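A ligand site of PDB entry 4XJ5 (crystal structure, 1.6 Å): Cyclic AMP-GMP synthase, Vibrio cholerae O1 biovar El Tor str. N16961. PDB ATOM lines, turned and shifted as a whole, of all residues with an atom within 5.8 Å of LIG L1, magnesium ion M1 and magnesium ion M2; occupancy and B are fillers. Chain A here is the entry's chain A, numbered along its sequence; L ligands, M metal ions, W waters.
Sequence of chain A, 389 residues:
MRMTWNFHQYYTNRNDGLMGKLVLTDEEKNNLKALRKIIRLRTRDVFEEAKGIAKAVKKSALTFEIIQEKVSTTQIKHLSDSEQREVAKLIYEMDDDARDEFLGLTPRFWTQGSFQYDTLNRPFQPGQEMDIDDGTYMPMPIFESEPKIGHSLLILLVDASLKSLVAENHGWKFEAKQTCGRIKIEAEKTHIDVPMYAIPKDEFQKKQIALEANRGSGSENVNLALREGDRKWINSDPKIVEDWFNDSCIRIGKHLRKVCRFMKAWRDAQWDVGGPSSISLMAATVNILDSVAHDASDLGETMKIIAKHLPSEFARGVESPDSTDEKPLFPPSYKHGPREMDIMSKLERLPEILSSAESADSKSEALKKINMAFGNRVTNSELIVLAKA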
ATOM      1  N   GLN A 112       8.257  11.002 -18.274  1.00  0.00           N
ATOM      2  CA  GLN A 112       9.585  11.513 -18.654  1.00  0.00           C
ATOM      3  C   GLN A 112       9.430  12.207 -19.989  1.00  0.00           C
ATOM      4  O   GLN A 112       8.351  12.201 -20.555  1.00  0.00           O
ATOM      5  CB  GLN A 112      10.608  10.372 -18.745  1.00  0.00           C
ATOM      6  CG  GLN A 112      10.312   9.327 -19.847  1.00  0.00           C
ATOM      7  CD  GLN A 112      11.143   8.063 -19.705  1.00  0.00           C
ATOM      8  OE1 GLN A 112      10.933   7.305 -18.766  1.00  0.00           O
ATOM      9  NE2 GLN A 112      12.063   7.814 -20.643  1.00  0.00           N
ATOM     10  N   GLY A 113      10.485  12.873 -20.482  1.00  0.00           N
ATOM     11  CA  GLY A 113      10.378  13.425 -21.825  1.00  0.00           C
ATOM     12  C   GLY A 113       9.629  14.747 -21.914  1.00  0.00           C
ATOM     13  O   GLY A 113       9.391  15.433 -20.905  1.00  0.00           O
ATOM     14  N   SER A 114       9.217  15.079 -23.136  1.00  0.00           N
ATOM     15  CA  SER A 114       8.731  16.419 -23.429  1.00  0.00           C
ATOM     16  C   SER A 114       7.393  16.801 -22.796  1.00  0.00           C
ATOM     17  O   SER A 114       7.117  17.973 -22.592  1.00  0.00           O
ATOM     18  CB  SER A 114       8.697  16.632 -24.971  1.00  0.00           C
ATOM     19  OG  SER A 114       7.797  15.758 -25.648  1.00  0.00           O
ATOM     20  N   ASP A 131       3.878  12.504 -28.683  1.00  0.00           N
ATOM     21  CA  ASP A 131       4.444  11.422 -27.872  1.00  0.00           C
ATOM     22  C   ASP A 131       4.292  11.723 -26.371  1.00  0.00           C
ATOM     23  O   ASP A 131       4.620  12.814 -25.928  1.00  0.00           O
ATOM     24  CB  ASP A 131       5.922  11.254 -28.265  1.00  0.00           C
ATOM     25  CG  ASP A 131       6.644  10.177 -27.487  1.00  0.00           C
ATOM     26  OD1 ASP A 131       6.119   9.046 -27.377  1.00  0.00           O
ATOM     27  OD2 ASP A 131       7.735  10.472 -26.982  1.00  0.00           O
ATOM     28  N   ILE A 132       3.804  10.758 -25.607  1.00  0.00           N
ATOM     29  CA  ILE A 132       3.791  10.853 -24.151  1.00  0.00           C
ATOM     30  C   ILE A 132       4.615   9.695 -23.635  1.00  0.00           C
ATOM     31  O   ILE A 132       4.307   8.556 -23.935  1.00  0.00           O
ATOM     32  CB  ILE A 132       2.396  10.721 -23.531  1.00  0.00           C
ATOM     33  CG1 ILE A 132       1.454  11.763 -24.108  1.00  0.00           C
ATOM     34  CG2 ILE A 132       2.509  10.848 -22.015  1.00  0.00           C
ATOM     35  CD1 ILE A 132       1.869  13.144 -23.792  1.00  0.00           C
ATOM     36  N   ASP A 133       5.676   9.992 -22.881  1.00  0.00           N
ATOM     37  CA  ASP A 133       6.537   8.945 -22.334  1.00  0.00           C
ATOM     38  C   ASP A 133       6.180   8.720 -20.879  1.00  0.00           C
ATOM     39  O   ASP A 133       6.605   9.462 -20.008  1.00  0.00           O
ATOM     40  CB  ASP A 133       7.996   9.359 -22.452  1.00  0.00           C
ATOM     41  CG  ASP A 133       8.420   9.605 -23.871  1.00  0.00           C
ATOM     42  OD1 ASP A 133       8.695   8.648 -24.588  1.00  0.00           O
ATOM     43  OD2 ASP A 133       8.571  10.783 -24.279  1.00  0.00           O
ATOM     44  N   ASP A 134       5.382   7.691 -20.587  1.00  0.00           N
ATOM     45  CA  ASP A 134       4.980   7.495 -19.206  1.00  0.00           C
ATOM     46  C   ASP A 134       5.558   6.188 -18.686  1.00  0.00           C
ATOM     47  O   ASP A 134       5.114   5.088 -19.047  1.00  0.00           O
ATOM     48  CB  ASP A 134       3.471   7.488 -19.058  1.00  0.00           C
ATOM     49  CG  ASP A 134       3.050   7.682 -17.612  1.00  0.00           C
ATOM     50  OD1 ASP A 134       3.561   8.623 -16.976  1.00  0.00           O
ATOM     51  OD2 ASP A 134       2.283   6.859 -17.075  1.00  0.00           O
ATOM     52  N   LYS A 177       8.448  -2.122 -28.684  1.00  0.00           N
ATOM     53  CA  LYS A 177       9.740  -1.528 -28.954  1.00  0.00           C
ATOM     54  C   LYS A 177      10.777  -2.087 -27.992  1.00  0.00           C
ATOM     55  O   LYS A 177      10.446  -2.718 -26.977  1.00  0.00           O
ATOM     56  CB  LYS A 177       9.677  -0.004 -28.817  1.00  0.00           C
ATOM     57  CG  LYS A 177       8.392   0.612 -29.361  1.00  0.00           C
ATOM     58  CD  LYS A 177       8.592   1.170 -30.727  1.00  0.00           C
ATOM     59  CE  LYS A 177       9.564   2.346 -30.672  1.00  0.00           C
ATOM     60  NZ  LYS A 177       9.992   2.733 -32.032  1.00  0.00           N
ATOM     61  N   THR A 179      12.648  -0.588 -25.935  1.00  0.00           N
ATOM     62  CA  THR A 179      12.693   0.117 -24.659  1.00  0.00           C
ATOM     63  C   THR A 179      11.313   0.371 -24.075  1.00  0.00           C
ATOM     64  O   THR A 179      11.192   0.939 -22.996  1.00  0.00           O
ATOM     65  CB  THR A 179      13.421   1.483 -24.782  1.00  0.00           C
ATOM     66  OG1 THR A 179      12.717   2.312 -25.714  1.00  0.00           O
ATOM     67  CG2 THR A 179      14.839   1.273 -25.310  1.00  0.00           C
ATOM     68  N   CYS A 180      10.264  -0.052 -24.784  1.00  0.00           N
ATOM     69  CA  CYS A 180       8.923   0.166 -24.263  1.00  0.00           C
ATOM     70  C   CYS A 180       7.850  -0.542 -25.065  1.00  0.00           C
ATOM     71  O   CYS A 180       8.080  -0.982 -26.181  1.00  0.00           O
ATOM     72  CB  CYS A 180       8.597   1.656 -24.236  1.00  0.00           C
ATOM     73  SG  CYS A 180       8.464   2.438 -25.871  1.00  0.00           S
ATOM     74  N   ARG A 182       4.162   0.458 -26.759  1.00  0.00           N
ATOM     75  CA  ARG A 182       3.609   1.688 -27.294  1.00  0.00           C
ATOM     76  C   ARG A 182       2.159   1.500 -27.708  1.00  0.00           C
ATOM     77  O   ARG A 182       1.836   0.488 -28.342  1.00  0.00           O
ATOM     78  CB  ARG A 182       4.433   2.150 -28.473  1.00  0.00           C
ATOM     79  CG  ARG A 182       3.820   3.328 -29.242  1.00  0.00           C
ATOM     80  CD  ARG A 182       4.741   3.824 -30.350  1.00  0.00           C
ATOM     81  NE  ARG A 182       5.936   4.471 -29.818  1.00  0.00           N
ATOM     82  CZ  ARG A 182       6.819   5.154 -30.546  1.00  0.00           C
ATOM     83  NH1 ARG A 182       6.651   5.291 -31.854  1.00  0.00           N
ATOM     84  NH2 ARG A 182       7.871   5.699 -29.965  1.00  0.00           N
ATOM     85  N   HIS A 191       0.763   8.894 -29.646  1.00  0.00           N
ATOM     86  CA  HIS A 191       1.107   7.606 -29.084  1.00  0.00           C
ATOM     87  C   HIS A 191       1.651   7.789 -27.661  1.00  0.00           C
ATOM     88  O   HIS A 191       2.199   8.844 -27.298  1.00  0.00           O
ATOM     89  CB  HIS A 191       2.092   6.831 -29.980  1.00  0.00           C
ATOM     90  CG  HIS A 191       3.396   7.519 -30.246  1.00  0.00           C
ATOM     91  ND1 HIS A 191       3.704   8.089 -31.463  1.00  0.00           N
ATOM     92  CD2 HIS A 191       4.501   7.660 -29.474  1.00  0.00           C
ATOM     93  CE1 HIS A 191       4.922   8.595 -31.417  1.00  0.00           C
ATOM     94  NE2 HIS A 191       5.431   8.349 -30.212  1.00  0.00           N
ATOM     95  N   ASP A 193       4.197   5.926 -24.988  1.00  0.00           N
ATOM     96  CA  ASP A 193       5.255   4.956 -24.700  1.00  0.00           C
ATOM     97  C   ASP A 193       5.306   4.632 -23.235  1.00  0.00           C
ATOM     98  O   ASP A 193       5.232   5.522 -22.372  1.00  0.00           O
ATOM     99  CB  ASP A 193       6.606   5.516 -25.118  1.00  0.00           C
ATOM    100  CG  ASP A 193       6.832   5.443 -26.608  1.00  0.00           C
ATOM    101  OD1 ASP A 193       6.160   4.657 -27.301  1.00  0.00           O
ATOM    102  OD2 ASP A 193       7.705   6.198 -27.086  1.00  0.00           O
ATOM    103  N   PRO A 195       7.909   2.926 -21.040  1.00  0.00           N
ATOM    104  CA  PRO A 195       9.131   2.244 -20.624  1.00  0.00           C
ATOM    105  C   PRO A 195       8.939   1.677 -19.227  1.00  0.00           C
ATOM    106  O   PRO A 195       8.161   2.229 -18.427  1.00  0.00           O
ATOM    107  CB  PRO A 195      10.194   3.355 -20.648  1.00  0.00           C
ATOM    108  CG  PRO A 195       9.413   4.639 -20.449  1.00  0.00           C
ATOM    109  CD  PRO A 195       8.073   4.396 -21.148  1.00  0.00           C
ATOM    110  N   TYR A 197      10.681   0.235 -15.567  1.00  0.00           N
ATOM    111  CA  TYR A 197      11.879   0.303 -14.741  1.00  0.00           C
ATOM    112  C   TYR A 197      11.798  -0.571 -13.520  1.00  0.00           C
ATOM    113  O   TYR A 197      10.730  -0.707 -12.931  1.00  0.00           O
ATOM    114  CB  TYR A 197      12.125   1.726 -14.273  1.00  0.00           C
ATOM    115  CG  TYR A 197      12.295   2.722 -15.378  1.00  0.00           C
ATOM    116  CD1 TYR A 197      13.553   2.997 -15.885  1.00  0.00           C
ATOM    117  CD2 TYR A 197      11.204   3.384 -15.914  1.00  0.00           C
ATOM    118  CE1 TYR A 197      13.737   3.914 -16.897  1.00  0.00           C
ATOM    119  CE2 TYR A 197      11.364   4.327 -16.921  1.00  0.00           C
ATOM    120  CZ  TYR A 197      12.640   4.563 -17.407  1.00  0.00           C
ATOM    121  OH  TYR A 197      12.816   5.513 -18.397  1.00  0.00           O
ATOM    122  N   LEU A 224      16.241   0.305 -16.578  1.00  0.00           N
ATOM    123  CA  LEU A 224      15.314   0.253 -17.698  1.00  0.00           C
ATOM    124  C   LEU A 224      15.299  -1.149 -18.297  1.00  0.00           C
ATOM    125  O   LEU A 224      16.349  -1.708 -18.638  1.00  0.00           O
ATOM    126  CB  LEU A 224      15.717   1.275 -18.781  1.00  0.00           C
ATOM    127  CG  LEU A 224      14.935   1.243 -20.100  1.00  0.00           C
ATOM    128  CD1 LEU A 224      13.510   1.711 -19.895  1.00  0.00           C
ATOM    129  CD2 LEU A 224      15.659   2.138 -21.166  1.00  0.00           C
ATOM    130  N   SER A 236      19.519   3.424 -16.626  1.00  0.00           N
ATOM    131  CA  SER A 236      19.234   4.635 -17.370  1.00  0.00           C
ATOM    132  C   SER A 236      18.119   5.420 -16.691  1.00  0.00           C
ATOM    133  O   SER A 236      16.940   5.216 -16.984  1.00  0.00           O
ATOM    134  CB  SER A 236      18.840   4.320 -18.813  1.00  0.00           C
ATOM    135  OG  SER A 236      18.843   5.517 -19.601  1.00  0.00           O
ATOM    136  N   ASP A 237      18.496   6.328 -15.789  1.00  0.00           N
ATOM    137  CA  ASP A 237      17.512   7.075 -14.990  1.00  0.00           C
ATOM    138  C   ASP A 237      17.028   8.284 -15.759  1.00  0.00           C
ATOM    139  O   ASP A 237      17.816   9.196 -15.998  1.00  0.00           O
ATOM    140  CB  ASP A 237      18.128   7.515 -13.667  1.00  0.00           C
ATOM    141  CG  ASP A 237      17.143   8.229 -12.770  1.00  0.00           C
ATOM    142  OD1 ASP A 237      15.953   8.321 -13.129  1.00  0.00           O
ATOM    143  OD2 ASP A 237      17.564   8.652 -11.677  1.00  0.00           O
ATOM    144  N   PRO A 238      15.743   8.318 -16.132  1.00  0.00           N
ATOM    145  CA  PRO A 238      15.308   9.484 -16.921  1.00  0.00           C
ATOM    146  C   PRO A 238      15.397  10.794 -16.148  1.00  0.00           C
ATOM    147  O   PRO A 238      15.418  11.859 -16.816  1.00  0.00           O
ATOM    148  CB  PRO A 238      13.845   9.156 -17.275  1.00  0.00           C
ATOM    149  CG  PRO A 238      13.414   8.120 -16.258  1.00  0.00           C
ATOM    150  CD  PRO A 238      14.666   7.322 -15.906  1.00  0.00           C
ATOM    151  N   ASP A 325      25.575   6.804 -20.792  1.00  0.00           N
ATOM    152  CA  ASP A 325      25.135   6.352 -22.104  1.00  0.00           C
ATOM    153  C   ASP A 325      26.310   5.761 -22.886  1.00  0.00           C
ATOM    154  O   ASP A 325      27.415   6.302 -22.853  1.00  0.00           O
ATOM    155  CB  ASP A 325      24.525   7.510 -22.914  1.00  0.00           C
ATOM    156  CG  ASP A 325      23.086   7.829 -22.528  1.00  0.00           C
ATOM    157  OD1 ASP A 325      22.603   7.295 -21.506  1.00  0.00           O
ATOM    158  OD2 ASP A 325      22.454   8.606 -23.266  1.00  0.00           O
HETATM  159  O1  LIG L   1      11.901   6.362 -29.640  1.00  0.00           O
HETATM  160  P1  LIG L   1      12.626   5.091 -29.035  1.00  0.00           P
HETATM  161  O2  LIG L   1      14.121   5.204 -29.178  1.00  0.00           O
HETATM  162  O3  LIG L   1      12.217   3.860 -29.791  1.00  0.00           O
HETATM  163  O4  LIG L   1      12.293   4.930 -27.475  1.00  0.00           O
HETATM  164  C1  LIG L   1      10.943   4.777 -27.043  1.00  0.00           C
HETATM  165  C2  LIG L   1      10.817   5.311 -25.599  1.00  0.00           C
HETATM  166  O5  LIG L   1      11.562   4.628 -24.749  1.00  0.00           O
HETATM  167  C3  LIG L   1      11.322   6.787 -25.470  1.00  0.00           C
HETATM  168  C4  LIG L   1      11.658   6.816 -23.965  1.00  0.00           C
HETATM  169  O6  LIG L   1      10.345   6.955 -23.281  1.00  0.00           O
HETATM  170  C5  LIG L   1      12.211   5.634 -23.702  1.00  0.00           C
HETATM  171  N1  LIG L   1      13.598   5.535 -23.972  1.00  0.00           N
HETATM  172  C6  LIG L   1      14.269   5.345 -25.158  1.00  0.00           C
HETATM  173  N2  LIG L   1      15.610   5.338 -24.905  1.00  0.00           N
HETATM  174  C7  LIG L   1      15.757   5.513 -23.577  1.00  0.00           C
HETATM  175  C8  LIG L   1      16.965   5.576 -22.706  1.00  0.00           C
HETATM  176  O7  LIG L   1      18.087   5.483 -23.178  1.00  0.00           O
HETATM  177  N3  LIG L   1      16.797   5.749 -21.333  1.00  0.00           N
HETATM  178  C9  LIG L   1      15.510   5.864 -20.750  1.00  0.00           C
HETATM  179  N4  LIG L   1      15.370   6.077 -19.355  1.00  0.00           N
HETATM  180  N5  LIG L   1      14.359   5.832 -21.587  1.00  0.00           N
HETATM  181  C10 LIG L   1      14.517   5.606 -23.004  1.00  0.00           C
HETATM  182  P1  LG2 L   2       9.632  14.387 -28.328  1.00  0.00           P
HETATM  183  O1  LG2 L   2      10.149  14.294 -29.728  1.00  0.00           O
HETATM  184  O2  LG2 L   2       8.702  15.504 -27.966  1.00  0.00           O
HETATM  185  O3  LG2 L   2       9.016  13.058 -27.923  1.00  0.00           O
HETATM  186  O4  LG2 L   2      10.848  14.641 -27.338  1.00  0.00           O
HETATM  187  P2  LG2 L   2      11.309  14.010 -25.929  1.00  0.00           P
HETATM  188  O5  LG2 L   2      12.045  15.081 -25.149  1.00  0.00           O
HETATM  189  O6  LG2 L   2      10.083  13.410 -25.232  1.00  0.00           O
HETATM  190  O7  LG2 L   2      12.258  12.843 -26.400  1.00  0.00           O
HETATM  191  P3  LG2 L   2      12.048  11.260 -26.455  1.00  0.00           P
HETATM  192  O8  LG2 L   2      12.911  10.716 -27.560  1.00  0.00           O
HETATM  193  O9  LG2 L   2      10.587  10.891 -26.622  1.00  0.00           O
HETATM  194  O10 LG2 L   2      12.677  10.727 -25.077  1.00  0.00           O
HETATM  195  C1  LG2 L   2      11.967  10.910 -23.861  1.00  0.00           C
HETATM  196  C2  LG2 L   2      12.934  10.673 -22.695  1.00  0.00           C
HETATM  197  O11 LG2 L   2      13.455   9.437 -22.775  1.00  0.00           O
HETATM  198  C3  LG2 L   2      14.140  11.635 -22.727  1.00  0.00           C
HETATM  199  C4  LG2 L   2      15.175  10.784 -21.964  1.00  0.00           C
HETATM  200  O12 LG2 L   2      14.824  10.956 -20.545  1.00  0.00           O
HETATM  201  C5  LG2 L   2      14.967   9.499 -22.332  1.00  0.00           C
HETATM  202  N1  LG2 L   2      15.706   9.187 -23.505  1.00  0.00           N
HETATM  203  C6  LG2 L   2      15.372   9.076 -24.811  1.00  0.00           C
HETATM  204  N2  LG2 L   2      16.495   8.792 -25.522  1.00  0.00           N
HETATM  205  C7  LG2 L   2      17.515   8.726 -24.632  1.00  0.00           C
HETATM  206  C8  LG2 L   2      18.987   8.463 -24.771  1.00  0.00           C
HETATM  207  O13 LG2 L   2      19.492   8.226 -25.836  1.00  0.00           O
HETATM  208  N3  LG2 L   2      19.773   8.443 -23.632  1.00  0.00           N
HETATM  209  C9  LG2 L   2      19.211   8.681 -22.350  1.00  0.00           C
HETATM  210  N4  LG2 L   2      20.013   8.679 -21.203  1.00  0.00           N
HETATM  211  N5  LG2 L   2      17.830   8.955 -22.214  1.00  0.00           N
HETATM  212  C10 LG2 L   2      17.007   8.964 -23.397  1.00  0.00           C
HETATM  213 MG    MG M   1       8.798  11.904 -26.112  1.00  0.00          MG
HETATM  214 MG    MG M   2       8.197   8.216 -26.731  1.00  0.00          MG
HETATM  215  O   HOH W   1       9.888   8.501 -28.104  1.00  0.00           O
HETATM  216  O   HOH W   2       7.361  13.109 -25.319  1.00  0.00           O
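N5 of LIG L1 sits at hydrogen-bond distance from NE2 of Gln 112 (3.2 Å). The side-chain carboxylate (OD2) of Asp 325 lies within hydrogen-bond range of a nitrogen (N3) of LG2 L2. An oxygen (O5) of LIG L1 lies within hydrogen-bond range of the side-chain hydroxyl (OG1) of Thr 179, at 2.8 Å. A nitrogen (N3) of LIG L1 sits at hydrogen-bond distance from the side-chain hydroxyl of Ser 236 (2.7 Å). O2 of LG2 L2 lies within hydrogen-bond range of OG of Ser 114 (2.5 Å). The side-chain amide nitrogen (NE2) of Gln 112 is in hydrogen-bond range of an oxygen (O11) of LG2 L2 (3.0 Å). O of Ser 236 is in hydrogen-bond range of N4 of LIG L1 (3.0 Å). An oxygen (O3) of LIG L1 lies within salt-bridge range of the side-chain amino group (NZ) of Lys 177, 3.4 Å away. The backbone NH (N) of Ser 114 is in hydrogen-bond range of an oxygen (O5) of LG2 L2, 3.5 Å away. The side-chain hydroxyl (OH) of Tyr 197 lies within hydrogen-bond range of a nitrogen (N4) of LIG L1 (2.8 Å). OD1 of Asp 133 lies close to O6 of LIG L1.
Of the 20 residues printed, 3 come within 4 Å of magnesium ion M2. Along chain A the residues within 4 Å of magnesium ion M2 span positions 131 to 193.
Merely in contact with LIG L1: Cys 180, Pro 195, Leu 224 and Pro 238. Hydrophobic or aromatic side chains within 4 Å of LIG L1: Pro 195, Tyr 197, Leu 224 and Pro 238. 11 residues have an atom within 4 Å of LIG L1: Gln 112, Asp 133, Lys 177, Thr 179, Cys 180, Asp 193, Pro 195, Tyr 197, Leu 224, Ser 236 and Pro 238. The nearest printed residue that does not touch LIG L1 is Arg 182 (4.1 Å).
N3 of LG2 L2 is in hydrogen-bond range of O7 of LIG L1.
Magnesium ion M1 is bound by OD2 of Asp 131 (2.0 Å), water W2 (2.0 Å), O9 of LG2 L2 (2.1 Å), O3 of LG2 L2 (2.2 Å), OD2 of Asp 133 (2.2 Å) and O6 of LG2 L2 (2.2 Å). Magnesium ion M1 has six donor atoms within binding distance.
Water W2 lies within hydrogen-bond range of the side-chain hydroxyl (OG) of Ser 114 (2.7 Å) and the backbone carbonyl oxygen (O) of Asp 131 (2.8 Å).
Magnesium ion M2 is bound by the side-chain carboxylate (OD2) of Asp 193 (2.1 Å), water W1 (2.2 Å), the side-chain carboxylate (OD1) of Asp 133 (2.2 Å), the side-chain carboxylate (OD2) of Asp 131 (2.3 Å) and the side-chain carboxylate (OD1) of Asp 131 (2.3 Å).
OD1 of Asp 131 sits close to NE2 of His 191 (3.0 Å). OD1 of Asp 193 is in salt-bridge range of NE of Arg 182. OH of Tyr 197 lies within hydrogen-bond range of OE1 of Gln 112. N of Asp 193 is in hydrogen-bond range of O of Ile 132. O of Asp 193 lies within hydrogen-bond range of N of Asp 134 (2.8 Å). The backbone carbonyl oxygen (O) of Asp 133 is in hydrogen-bond range of the backbone NH (N) of Gln 112, 2.8 Å away. OD1 of Asp 193 sits close to SG of Cys 180 (3.5 Å).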
